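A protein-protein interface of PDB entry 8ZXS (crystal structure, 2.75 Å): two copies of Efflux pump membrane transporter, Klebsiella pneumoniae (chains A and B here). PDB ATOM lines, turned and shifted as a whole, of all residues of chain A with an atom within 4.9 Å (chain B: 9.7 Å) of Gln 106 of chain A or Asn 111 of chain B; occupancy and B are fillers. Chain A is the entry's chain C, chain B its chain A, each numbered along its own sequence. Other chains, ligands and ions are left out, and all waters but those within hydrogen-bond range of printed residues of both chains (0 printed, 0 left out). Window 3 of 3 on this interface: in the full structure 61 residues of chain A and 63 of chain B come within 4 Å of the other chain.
Of chain B, only Asn 111 (3.9 Å) comes within 4 Å of Gln 106 of chain A. Val 109 of chain A touches none of the printed residues of chain B. Thr 131 of chain A touches one residue of chain B. Printed residues of chain A within 4 Å of Glu 75 of chain B: Lys 133. Gln 106 of chain B touches none of the printed residues of chain A. Asn 111 of chain B touches three residues of chain A. Printed residues of chain A within 4 Å of Gln 115 of chain B: Gln 132 (3.96 Å). Thr 131 of chain B touches none of the printed residues of chain A. The nearest printed residue of chain B that does not touch Gln 106 of chain A is Val 107 of chain B (5.4 Å). The nearest printed residue of chain B that does not touch Asp 103 of chain A is Glu 75 of chain B (4.9 Å).
Gln 106 of chain A touches Asn 111 of chain B. NE2 of Gln 115 of chain B touches NE2 of Gln 132 of chain A (3.96 Å).
The side-chain carboxylate (OE2) of Glu 75 of chain B lies within salt-bridge range of the side-chain amino group (NZ) of Lys 133 of chain A (3.0 Å). The side-chain amide nitrogen (NE2) of Gln 104 of chain B is in hydrogen-bond range of the side-chain carboxylate (OD1) of Asp 103 of chain A (2.8 Å). The side-chain amide oxygen of Gln 110 of chain A is in hydrogen-bond range of the side-chain amide nitrogen of Asn 111 of chain B (2.9 Å). The side-chain amide nitrogen (ND2) of Asn 111 of chain B lies within hydrogen-bond range of the backbone carbonyl oxygen (O) of Thr 131 of chain A, 3.4 Å away.
Asp 103 of chain A touches Gln 104 of chain B, but with the chains exchanged Gln 104 of chain A does not touch Asp 103 of chain B (10.7 Å). 10 positions are printed for both chains.
Along chain B the printed residues that touch a printed residue of chain A span positions 75 to 115. Among the printed residues, Asp or Glu carboxylates within 4 Å of a Lys or Arg side-chain nitrogen of the other chain: Lys 133 of chain A with Glu 75 of chain B.
The side-chain amide oxygen (OD1) of Asn 111 of chain B sits close to the backbone carbonyl oxygen (O) of Val 107 of chain B. OD2 of Asp 103 of chain A lies within salt-bridge range of NZ of Lys 133 of chain A (3.8 Å). The side-chain amide oxygen (OE1) of Gln 110 of chain A sits at hydrogen-bond distance from the side-chain amide nitrogen (NE2) of Gln 106 of chain A, at 3.2 Å. The side-chain amide nitrogen of Gln 106 of chain A lies within hydrogen-bond range of the backbone carbonyl oxygen of Thr 131 of chain A (2.5 Å).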
ATOM      1  N   VAL A  45      29.977   9.863 -10.540  1.00  0.00           N
ATOM      2  CA  VAL A  45      28.595  10.317 -10.421  1.00  0.00           C
ATOM      3  C   VAL A  45      27.696   9.286 -11.084  1.00  0.00           C
ATOM      4  O   VAL A  45      27.992   8.816 -12.188  1.00  0.00           O
ATOM      5  CB  VAL A  45      28.390  11.704 -11.056  1.00  0.00           C
ATOM      6  CG1 VAL A  45      26.955  12.143 -10.884  1.00  0.00           C
ATOM      7  CG2 VAL A  45      29.338  12.724 -10.434  1.00  0.00           C
ATOM      8  N   PRO A 102      34.028  16.322  -6.266  1.00  0.00           N
ATOM      9  CA  PRO A 102      32.837  15.526  -6.606  1.00  0.00           C
ATOM     10  C   PRO A 102      31.561  16.343  -6.640  1.00  0.00           C
ATOM     11  O   PRO A 102      30.639  16.000  -7.389  1.00  0.00           O
ATOM     12  CB  PRO A 102      32.801  14.457  -5.504  1.00  0.00           C
ATOM     13  CG  PRO A 102      33.620  15.018  -4.390  1.00  0.00           C
ATOM     14  CD  PRO A 102      34.677  15.861  -5.029  1.00  0.00           C
ATOM     15  N   ASP A 103      31.485  17.423  -5.862  1.00  0.00           N
ATOM     16  CA  ASP A 103      30.275  18.241  -5.824  1.00  0.00           C
ATOM     17  C   ASP A 103      30.092  19.025  -7.118  1.00  0.00           C
ATOM     18  O   ASP A 103      28.987  19.074  -7.678  1.00  0.00           O
ATOM     19  CB  ASP A 103      30.332  19.179  -4.621  1.00  0.00           C
ATOM     20  CG  ASP A 103      30.272  18.431  -3.306  1.00  0.00           C
ATOM     21  OD1 ASP A 103      29.385  17.564  -3.167  1.00  0.00           O
ATOM     22  OD2 ASP A 103      31.108  18.703  -2.418  1.00  0.00           O
ATOM     23  N   GLN A 104      31.167  19.649  -7.606  1.00  0.00           N
ATOM     24  CA  GLN A 104      31.102  20.355  -8.881  1.00  0.00           C
ATOM     25  C   GLN A 104      30.759  19.400 -10.019  1.00  0.00           C
ATOM     26  O   GLN A 104      29.941  19.725 -10.891  1.00  0.00           O
ATOM     27  CB  GLN A 104      32.431  21.059  -9.150  1.00  0.00           C
ATOM     28  CG  GLN A 104      32.499  21.750 -10.500  1.00  0.00           C
ATOM     29  CD  GLN A 104      32.710  23.244 -10.372  1.00  0.00           C
ATOM     30  OE1 GLN A 104      32.752  23.784  -9.264  1.00  0.00           O
ATOM     31  NE2 GLN A 104      32.842  23.923 -11.505  1.00  0.00           N
ATOM     32  N   ALA A 105      31.375  18.216 -10.022  1.00  0.00           N
ATOM     33  CA  ALA A 105      31.052  17.216 -11.031  1.00  0.00           C
ATOM     34  C   ALA A 105      29.587  16.821 -10.957  1.00  0.00           C
ATOM     35  O   ALA A 105      28.920  16.681 -11.991  1.00  0.00           O
ATOM     36  CB  ALA A 105      31.942  15.987 -10.855  1.00  0.00           C
ATOM     37  N   GLN A 106      29.070  16.630  -9.741  1.00  0.00           N
ATOM     38  CA  GLN A 106      27.666  16.279  -9.587  1.00  0.00           C
ATOM     39  C   GLN A 106      26.778  17.348 -10.197  1.00  0.00           C
ATOM     40  O   GLN A 106      25.872  17.042 -10.979  1.00  0.00           O
ATOM     41  CB  GLN A 106      27.329  16.084  -8.107  1.00  0.00           C
ATOM     42  CG  GLN A 106      26.023  15.334  -7.857  1.00  0.00           C
ATOM     43  CD  GLN A 106      24.792  16.219  -7.981  1.00  0.00           C
ATOM     44  OE1 GLN A 106      24.874  17.444  -7.869  1.00  0.00           O
ATOM     45  NE2 GLN A 106      23.640  15.598  -8.201  1.00  0.00           N
ATOM     46  N   VAL A 107      27.040  18.614  -9.864  1.00  0.00           N
ATOM     47  CA  VAL A 107      26.185  19.696 -10.345  1.00  0.00           C
ATOM     48  C   VAL A 107      26.236  19.792 -11.865  1.00  0.00           C
ATOM     49  O   VAL A 107      25.209  20.001 -12.522  1.00  0.00           O
ATOM     50  CB  VAL A 107      26.567  21.029  -9.678  1.00  0.00           C
ATOM     51  CG1 VAL A 107      25.652  22.140 -10.170  1.00  0.00           C
ATOM     52  CG2 VAL A 107      26.471  20.906  -8.166  1.00  0.00           C
ATOM     53  N   GLN A 108      27.426  19.643 -12.452  1.00  0.00           N
ATOM     54  CA  GLN A 108      27.543  19.756 -13.903  1.00  0.00           C
ATOM     55  C   GLN A 108      26.832  18.607 -14.615  1.00  0.00           C
ATOM     56  O   GLN A 108      26.092  18.824 -15.587  1.00  0.00           O
ATOM     57  CB  GLN A 108      29.016  19.817 -14.299  1.00  0.00           C
ATOM     58  CG  GLN A 108      29.710  21.079 -13.818  1.00  0.00           C
ATOM     59  CD  GLN A 108      31.041  21.302 -14.493  1.00  0.00           C
ATOM     60  OE1 GLN A 108      31.682  20.358 -14.948  1.00  0.00           O
ATOM     61  NE2 GLN A 108      31.469  22.557 -14.557  1.00  0.00           N
ATOM     62  N   VAL A 109      27.042  17.374 -14.146  1.00  0.00           N
ATOM     63  CA  VAL A 109      26.342  16.235 -14.730  1.00  0.00           C
ATOM     64  C   VAL A 109      24.838  16.419 -14.592  1.00  0.00           C
ATOM     65  O   VAL A 109      24.070  16.102 -15.509  1.00  0.00           O
ATOM     66  CB  VAL A 109      26.818  14.923 -14.076  1.00  0.00           C
ATOM     67  CG1 VAL A 109      25.940  13.750 -14.503  1.00  0.00           C
ATOM     68  CG2 VAL A 109      28.279  14.659 -14.411  1.00  0.00           C
ATOM     69  N   GLN A 110      24.395  16.944 -13.447  1.00  0.00           N
ATOM     70  CA  GLN A 110      22.972  17.173 -13.228  1.00  0.00           C
ATOM     71  C   GLN A 110      22.418  18.186 -14.220  1.00  0.00           C
ATOM     72  O   GLN A 110      21.361  17.968 -14.825  1.00  0.00           O
ATOM     73  CB  GLN A 110      22.742  17.645 -11.795  1.00  0.00           C
ATOM     74  CG  GLN A 110      21.343  18.132 -11.551  1.00  0.00           C
ATOM     75  CD  GLN A 110      20.909  17.953 -10.122  1.00  0.00           C
ATOM     76  OE1 GLN A 110      21.067  16.876  -9.547  1.00  0.00           O
ATOM     77  NE2 GLN A 110      20.341  19.006  -9.539  1.00  0.00           N
ATOM     78  N   THR A 131      20.522  11.995 -10.232  1.00  0.00           N
ATOM     79  CA  THR A 131      21.956  12.228 -10.397  1.00  0.00           C
ATOM     80  C   THR A 131      22.572  12.440  -9.019  1.00  0.00           C
ATOM     81  O   THR A 131      22.371  13.488  -8.397  1.00  0.00           O
ATOM     82  CB  THR A 131      22.219  13.421 -11.321  1.00  0.00           C
ATOM     83  OG1 THR A 131      21.740  13.111 -12.636  1.00  0.00           O
ATOM     84  CG2 THR A 131      23.698  13.739 -11.403  1.00  0.00           C
ATOM     85  N   GLN A 132      23.310  11.441  -8.539  1.00  0.00           N
ATOM     86  CA  GLN A 132      23.952  11.510  -7.231  1.00  0.00           C
ATOM     87  C   GLN A 132      25.431  11.215  -7.382  1.00  0.00           C
ATOM     88  O   GLN A 132      25.804  10.260  -8.066  1.00  0.00           O
ATOM     89  CB  GLN A 132      23.344  10.513  -6.238  1.00  0.00           C
ATOM     90  CG  GLN A 132      21.907  10.117  -6.517  1.00  0.00           C
ATOM     91  CD  GLN A 132      21.524   8.817  -5.830  1.00  0.00           C
ATOM     92  OE1 GLN A 132      22.388   8.053  -5.402  1.00  0.00           O
ATOM     93  NE2 GLN A 132      20.224   8.569  -5.711  1.00  0.00           N
ATOM     94  N   LYS A 133      26.275  12.020  -6.744  1.00  0.00           N
ATOM     95  CA  LYS A 133      27.670  11.627  -6.618  1.00  0.00           C
ATOM     96  C   LYS A 133      27.738  10.351  -5.793  1.00  0.00           C
ATOM     97  O   LYS A 133      27.005  10.190  -4.814  1.00  0.00           O
ATOM     98  CB  LYS A 133      28.496  12.750  -5.984  1.00  0.00           C
ATOM     99  CG  LYS A 133      28.507  12.775  -4.470  1.00  0.00           C
ATOM    100  CD  LYS A 133      29.017  14.098  -3.939  1.00  0.00           C
ATOM    101  CE  LYS A 133      28.511  14.320  -2.527  1.00  0.00           C
ATOM    102  NZ  LYS A 133      28.702  15.720  -2.079  1.00  0.00           N
ATOM    103  N   VAL B  45      17.519  24.765   5.371  1.00  0.00           N
ATOM    104  CA  VAL B  45      16.756  24.734   4.132  1.00  0.00           C
ATOM    105  C   VAL B  45      15.307  24.422   4.477  1.00  0.00           C
ATOM    106  O   VAL B  45      15.030  23.478   5.228  1.00  0.00           O
ATOM    107  CB  VAL B  45      17.328  23.705   3.141  1.00  0.00           C
ATOM    108  CG1 VAL B  45      16.375  23.497   1.980  1.00  0.00           C
ATOM    109  CG2 VAL B  45      18.696  24.158   2.647  1.00  0.00           C
ATOM    110  N   VAL B  47      11.518  23.406   3.195  1.00  0.00           N
ATOM    111  CA  VAL B  47      10.717  22.750   2.170  1.00  0.00           C
ATOM    112  C   VAL B  47       9.256  22.995   2.518  1.00  0.00           C
ATOM    113  O   VAL B  47       8.799  22.610   3.601  1.00  0.00           O
ATOM    114  CB  VAL B  47      11.023  21.247   2.093  1.00  0.00           C
ATOM    115  CG1 VAL B  47      10.175  20.581   1.026  1.00  0.00           C
ATOM    116  CG2 VAL B  47      12.479  21.033   1.813  1.00  0.00           C
ATOM    117  N   LEU B  67       8.037  12.518   2.183  1.00  0.00           N
ATOM    118  CA  LEU B  67       9.122  13.480   2.049  1.00  0.00           C
ATOM    119  C   LEU B  67      10.268  13.103   2.976  1.00  0.00           C
ATOM    120  O   LEU B  67      11.368  12.776   2.522  1.00  0.00           O
ATOM    121  CB  LEU B  67       8.622  14.893   2.353  1.00  0.00           C
ATOM    122  CG  LEU B  67       7.890  15.639   1.235  1.00  0.00           C
ATOM    123  CD1 LEU B  67       7.439  17.011   1.711  1.00  0.00           C
ATOM    124  CD2 LEU B  67       8.766  15.765  -0.001  1.00  0.00           C
ATOM    125  N   ALA B  70      12.385  10.561   2.078  1.00  0.00           N
ATOM    126  CA  ALA B  70      13.300  10.880   0.983  1.00  0.00           C
ATOM    127  C   ALA B  70      14.485  11.732   1.439  1.00  0.00           C
ATOM    128  O   ALA B  70      15.629  11.458   1.056  1.00  0.00           O
ATOM    129  CB  ALA B  70      12.556  11.578  -0.154  1.00  0.00           C
ATOM    130  N   ILE B  71      14.240  12.786   2.227  1.00  0.00           N
ATOM    131  CA  ILE B  71      15.352  13.686   2.539  1.00  0.00           C
ATOM    132  C   ILE B  71      16.313  13.081   3.555  1.00  0.00           C
ATOM    133  O   ILE B  71      17.461  13.532   3.651  1.00  0.00           O
ATOM    134  CB  ILE B  71      14.910  15.091   3.036  1.00  0.00           C
ATOM    135  CG1 ILE B  71      13.706  15.678   2.295  1.00  0.00           C
ATOM    136  CG2 ILE B  71      16.044  16.102   2.984  1.00  0.00           C
ATOM    137  CD1 ILE B  71      12.417  15.529   3.032  1.00  0.00           C
ATOM    138  N   ASN B  72      15.885  12.078   4.315  1.00  0.00           N
ATOM    139  CA  ASN B  72      16.738  11.534   5.363  1.00  0.00           C
ATOM    140  C   ASN B  72      18.026  10.961   4.785  1.00  0.00           C
ATOM    141  O   ASN B  72      18.023  10.296   3.744  1.00  0.00           O
ATOM    142  CB  ASN B  72      15.999  10.452   6.148  1.00  0.00           C
ATOM    143  CG  ASN B  72      16.792   9.966   7.329  1.00  0.00           C
ATOM    144  OD1 ASN B  72      16.915  10.664   8.335  1.00  0.00           O
ATOM    145  ND2 ASN B  72      17.351   8.765   7.212  1.00  0.00           N
ATOM    146  N   VAL B  74      20.548  13.050   3.920  1.00  0.00           N
ATOM    147  CA  VAL B  74      21.180  14.064   3.084  1.00  0.00           C
ATOM    148  C   VAL B  74      22.503  14.505   3.717  1.00  0.00           C
ATOM    149  O   VAL B  74      22.677  14.482   4.943  1.00  0.00           O
ATOM    150  CB  VAL B  74      20.226  15.253   2.849  1.00  0.00           C
ATOM    151  CG1 VAL B  74      20.308  16.269   3.973  1.00  0.00           C
ATOM    152  CG2 VAL B  74      20.512  15.928   1.518  1.00  0.00           C
ATOM    153  N   GLU B  75      23.456  14.875   2.864  1.00  0.00           N
ATOM    154  CA  GLU B  75      24.814  15.149   3.315  1.00  0.00           C
ATOM    155  C   GLU B  75      24.862  16.365   4.234  1.00  0.00           C
ATOM    156  O   GLU B  75      24.222  17.387   3.973  1.00  0.00           O
ATOM    157  CB  GLU B  75      25.730  15.363   2.109  1.00  0.00           C
ATOM    158  CG  GLU B  75      27.100  15.908   2.451  1.00  0.00           C
ATOM    159  CD  GLU B  75      28.157  15.504   1.446  1.00  0.00           C
ATOM    160  OE1 GLU B  75      29.267  16.075   1.487  1.00  0.00           O
ATOM    161  OE2 GLU B  75      27.878  14.610   0.620  1.00  0.00           O
ATOM    162  N   ASP B 103      23.920  26.699  -0.577  1.00  0.00           N
ATOM    163  CA  ASP B 103      23.441  26.406  -1.926  1.00  0.00           C
ATOM    164  C   ASP B 103      23.532  24.916  -2.231  1.00  0.00           C
ATOM    165  O   ASP B 103      22.616  24.332  -2.827  1.00  0.00           O
ATOM    166  CB  ASP B 103      24.236  27.215  -2.951  1.00  0.00           C
ATOM    167  CG  ASP B 103      24.261  28.697  -2.632  1.00  0.00           C
ATOM    168  OD1 ASP B 103      23.630  29.103  -1.634  1.00  0.00           O
ATOM    169  OD2 ASP B 103      24.914  29.457  -3.379  1.00  0.00           O
ATOM    170  N   GLN B 104      24.638  24.284  -1.835  1.00  0.00           N
ATOM    171  CA  GLN B 104      24.782  22.847  -2.032  1.00  0.00           C
ATOM    172  C   GLN B 104      23.744  22.080  -1.229  1.00  0.00           C
ATOM    173  O   GLN B 104      23.162  21.097  -1.713  1.00  0.00           O
ATOM    174  CB  GLN B 104      26.195  22.409  -1.648  1.00  0.00           C
ATOM    175  CG  GLN B 104      26.434  20.933  -1.841  1.00  0.00           C
ATOM    176  CD  GLN B 104      27.508  20.663  -2.866  1.00  0.00           C
ATOM    177  OE1 GLN B 104      28.409  21.478  -3.077  1.00  0.00           O
ATOM    178  NE2 GLN B 104      27.399  19.524  -3.540  1.00  0.00           N
ATOM    179  N   ALA B 105      23.499  22.512   0.006  1.00  0.00           N
ATOM    180  CA  ALA B 105      22.462  21.876   0.801  1.00  0.00           C
ATOM    181  C   ALA B 105      21.115  21.986   0.105  1.00  0.00           C
ATOM    182  O   ALA B 105      20.358  21.010   0.040  1.00  0.00           O
ATOM    183  CB  ALA B 105      22.413  22.504   2.193  1.00  0.00           C
ATOM    184  N   GLN B 106      20.817  23.161  -0.452  1.00  0.00           N
ATOM    185  CA  GLN B 106      19.541  23.366  -1.126  1.00  0.00           C
ATOM    186  C   GLN B 106      19.400  22.461  -2.344  1.00  0.00           C
ATOM    187  O   GLN B 106      18.337  21.864  -2.559  1.00  0.00           O
ATOM    188  CB  GLN B 106      19.395  24.832  -1.523  1.00  0.00           C
ATOM    189  CG  GLN B 106      18.149  25.140  -2.321  1.00  0.00           C
ATOM    190  CD  GLN B 106      18.320  26.372  -3.177  1.00  0.00           C
ATOM    191  OE1 GLN B 106      18.232  27.498  -2.685  1.00  0.00           O
ATOM    192  NE2 GLN B 106      18.582  26.169  -4.467  1.00  0.00           N
ATOM    193  N   VAL B 107      20.457  22.341  -3.151  1.00  0.00           N
ATOM    194  CA  VAL B 107      20.346  21.501  -4.341  1.00  0.00           C
ATOM    195  C   VAL B 107      20.181  20.034  -3.946  1.00  0.00           C
ATOM    196  O   VAL B 107      19.407  19.298  -4.570  1.00  0.00           O
ATOM    197  CB  VAL B 107      21.533  21.716  -5.304  1.00  0.00           C
ATOM    198  CG1 VAL B 107      21.586  23.164  -5.779  1.00  0.00           C
ATOM    199  CG2 VAL B 107      22.842  21.317  -4.687  1.00  0.00           C
ATOM    200  N   GLN B 108      20.868  19.588  -2.890  1.00  0.00           N
ATOM    201  CA  GLN B 108      20.692  18.201  -2.459  1.00  0.00           C
ATOM    202  C   GLN B 108      19.283  17.953  -1.931  1.00  0.00           C
ATOM    203  O   GLN B 108      18.661  16.920  -2.237  1.00  0.00           O
ATOM    204  CB  GLN B 108      21.733  17.842  -1.401  1.00  0.00           C
ATOM    205  CG  GLN B 108      23.165  17.933  -1.895  1.00  0.00           C
ATOM    206  CD  GLN B 108      24.147  17.293  -0.939  1.00  0.00           C
ATOM    207  OE1 GLN B 108      24.154  16.075  -0.758  1.00  0.00           O
ATOM    208  NE2 GLN B 108      24.984  18.116  -0.315  1.00  0.00           N
ATOM    209  N   VAL B 109      18.756  18.893  -1.143  1.00  0.00           N
ATOM    210  CA  VAL B 109      17.412  18.721  -0.603  1.00  0.00           C
ATOM    211  C   VAL B 109      16.387  18.700  -1.729  1.00  0.00           C
ATOM    212  O   VAL B 109      15.468  17.872  -1.727  1.00  0.00           O
ATOM    213  CB  VAL B 109      17.093  19.811   0.435  1.00  0.00           C
ATOM    214  CG1 VAL B 109      15.682  19.631   0.950  1.00  0.00           C
ATOM    215  CG2 VAL B 109      18.072  19.742   1.591  1.00  0.00           C
ATOM    216  N   GLN B 110      16.528  19.591  -2.717  1.00  0.00           N
ATOM    217  CA  GLN B 110      15.561  19.554  -3.809  1.00  0.00           C
ATOM    218  C   GLN B 110      15.727  18.301  -4.660  1.00  0.00           C
ATOM    219  O   GLN B 110      14.742  17.811  -5.214  1.00  0.00           O
ATOM    220  CB  GLN B 110      15.622  20.798  -4.696  1.00  0.00           C
ATOM    221  CG  GLN B 110      14.272  20.936  -5.452  1.00  0.00           C
ATOM    222  CD  GLN B 110      14.245  21.956  -6.578  1.00  0.00           C
ATOM    223  OE1 GLN B 110      14.211  23.166  -6.345  1.00  0.00           O
ATOM    224  NE2 GLN B 110      14.232  21.461  -7.814  1.00  0.00           N
ATOM    225  N   ASN B 111      16.944  17.754  -4.757  1.00  0.00           N
ATOM    226  CA  ASN B 111      17.115  16.457  -5.402  1.00  0.00           C
ATOM    227  C   ASN B 111      16.262  15.398  -4.717  1.00  0.00           C
ATOM    228  O   ASN B 111      15.546  14.624  -5.371  1.00  0.00           O
ATOM    229  CB  ASN B 111      18.589  16.049  -5.372  1.00  0.00           C
ATOM    230  CG  ASN B 111      19.333  16.448  -6.631  1.00  0.00           C
ATOM    231  OD1 ASN B 111      19.461  17.633  -6.943  1.00  0.00           O
ATOM    232  ND2 ASN B 111      19.830  15.455  -7.362  1.00  0.00           N
ATOM    233  N   ARG B 112      16.311  15.370  -3.385  1.00  0.00           N
ATOM    234  CA  ARG B 112      15.562  14.344  -2.665  1.00  0.00           C
ATOM    235  C   ARG B 112      14.053  14.596  -2.716  1.00  0.00           C
ATOM    236  O   ARG B 112      13.265  13.645  -2.822  1.00  0.00           O
ATOM    237  CB  ARG B 112      16.077  14.235  -1.232  1.00  0.00           C
ATOM    238  CG  ARG B 112      17.448  13.579  -1.185  1.00  0.00           C
ATOM    239  CD  ARG B 112      18.071  13.610   0.187  1.00  0.00           C
ATOM    240  NE  ARG B 112      18.587  12.300   0.569  1.00  0.00           N
ATOM    241  CZ  ARG B 112      19.863  11.948   0.489  1.00  0.00           C
ATOM    242  NH1 ARG B 112      20.784  12.782   0.029  1.00  0.00           N
ATOM    243  NH2 ARG B 112      20.226  10.730   0.881  1.00  0.00           N
ATOM    244  N   VAL B 113      13.620  15.861  -2.674  1.00  0.00           N
ATOM    245  CA  VAL B 113      12.182  16.096  -2.823  1.00  0.00           C
ATOM    246  C   VAL B 113      11.736  15.771  -4.244  1.00  0.00           C
ATOM    247  O   VAL B 113      10.595  15.348  -4.456  1.00  0.00           O
ATOM    248  CB  VAL B 113      11.754  17.527  -2.414  1.00  0.00           C
ATOM    249  CG1 VAL B 113      12.418  17.955  -1.118  1.00  0.00           C
ATOM    250  CG2 VAL B 113      12.006  18.540  -3.530  1.00  0.00           C
ATOM    251  N   ALA B 114      12.610  15.961  -5.236  1.00  0.00           N
ATOM    252  CA  ALA B 114      12.266  15.590  -6.602  1.00  0.00           C
ATOM    253  C   ALA B 114      12.062  14.091  -6.716  1.00  0.00           C
ATOM    254  O   ALA B 114      11.146  13.630  -7.405  1.00  0.00           O
ATOM    255  CB  ALA B 114      13.353  16.056  -7.567  1.00  0.00           C
ATOM    256  N   GLN B 115      12.915  13.315  -6.049  1.00  0.00           N
ATOM    257  CA  GLN B 115      12.672  11.879  -5.993  1.00  0.00           C
ATOM    258  C   GLN B 115      11.362  11.572  -5.278  1.00  0.00           C
ATOM    259  O   GLN B 115      10.656  10.625  -5.644  1.00  0.00           O
ATOM    260  CB  GLN B 115      13.839  11.165  -5.309  1.00  0.00           C
ATOM    261  CG  GLN B 115      15.198  11.491  -5.905  1.00  0.00           C
ATOM    262  CD  GLN B 115      16.331  10.772  -5.199  1.00  0.00           C
ATOM    263  OE1 GLN B 115      16.157   9.671  -4.678  1.00  0.00           O
ATOM    264  NE2 GLN B 115      17.504  11.398  -5.176  1.00  0.00           N
ATOM    265  N   ALA B 116      11.018  12.366  -4.258  1.00  0.00           N
ATOM    266  CA  ALA B 116       9.842  12.078  -3.438  1.00  0.00           C
ATOM    267  C   ALA B 116       8.520  12.452  -4.104  1.00  0.00           C
ATOM    268  O   ALA B 116       7.484  11.858  -3.782  1.00  0.00           O
ATOM    269  CB  ALA B 116       9.945  12.810  -2.103  1.00  0.00           C
ATOM    270  N   GLU B 117       8.530  13.430  -5.013  1.00  0.00           N
ATOM    271  CA  GLU B 117       7.288  14.034  -5.489  1.00  0.00           C
ATOM    272  C   GLU B 117       6.359  13.044  -6.182  1.00  0.00           C
ATOM    273  O   GLU B 117       5.162  13.327  -6.306  1.00  0.00           O
ATOM    274  CB  GLU B 117       7.599  15.198  -6.434  1.00  0.00           C
ATOM    275  CG  GLU B 117       7.640  16.543  -5.730  1.00  0.00           C
ATOM    276  CD  GLU B 117       7.985  17.710  -6.642  1.00  0.00           C
ATOM    277  OE1 GLU B 117       9.189  17.960  -6.866  1.00  0.00           O
ATOM    278  OE2 GLU B 117       7.051  18.390  -7.118  1.00  0.00           O
ATOM    279  N   ALA B 118       6.869  11.898  -6.632  1.00  0.00           N
ATOM    280  CA  ALA B 118       6.025  10.955  -7.360  1.00  0.00           C
ATOM    281  C   ALA B 118       4.976  10.306  -6.461  1.00  0.00           C
ATOM    282  O   ALA B 118       3.900   9.933  -6.942  1.00  0.00           O
ATOM    283  CB  ALA B 118       6.889   9.880  -8.021  1.00  0.00           C
ATOM    284  N   ILE B 129       5.932  22.126  -4.598  1.00  0.00           N
ATOM    285  CA  ILE B 129       6.539  22.217  -3.277  1.00  0.00           C
ATOM    286  C   ILE B 129       7.905  22.861  -3.433  1.00  0.00           C
ATOM    287  O   ILE B 129       8.703  22.438  -4.276  1.00  0.00           O
ATOM    288  CB  ILE B 129       6.649  20.843  -2.591  1.00  0.00           C
ATOM    289  CG1 ILE B 129       7.174  19.782  -3.540  1.00  0.00           C
ATOM    290  CG2 ILE B 129       5.280  20.379  -2.183  1.00  0.00           C
ATOM    291  CD1 ILE B 129       7.098  18.414  -2.924  1.00  0.00           C
ATOM    292  N   THR B 131      11.624  24.338  -2.331  1.00  0.00           N
ATOM    293  CA  THR B 131      12.800  24.126  -1.496  1.00  0.00           C
ATOM    294  C   THR B 131      13.677  25.367  -1.589  1.00  0.00           C
ATOM    295  O   THR B 131      14.056  25.775  -2.691  1.00  0.00           O
ATOM    296  CB  THR B 131      13.577  22.886  -1.947  1.00  0.00           C
ATOM    297  OG1 THR B 131      12.675  21.798  -2.194  1.00  0.00           O
ATOM    298  CG2 THR B 131      14.573  22.475  -0.891  1.00  0.00           C
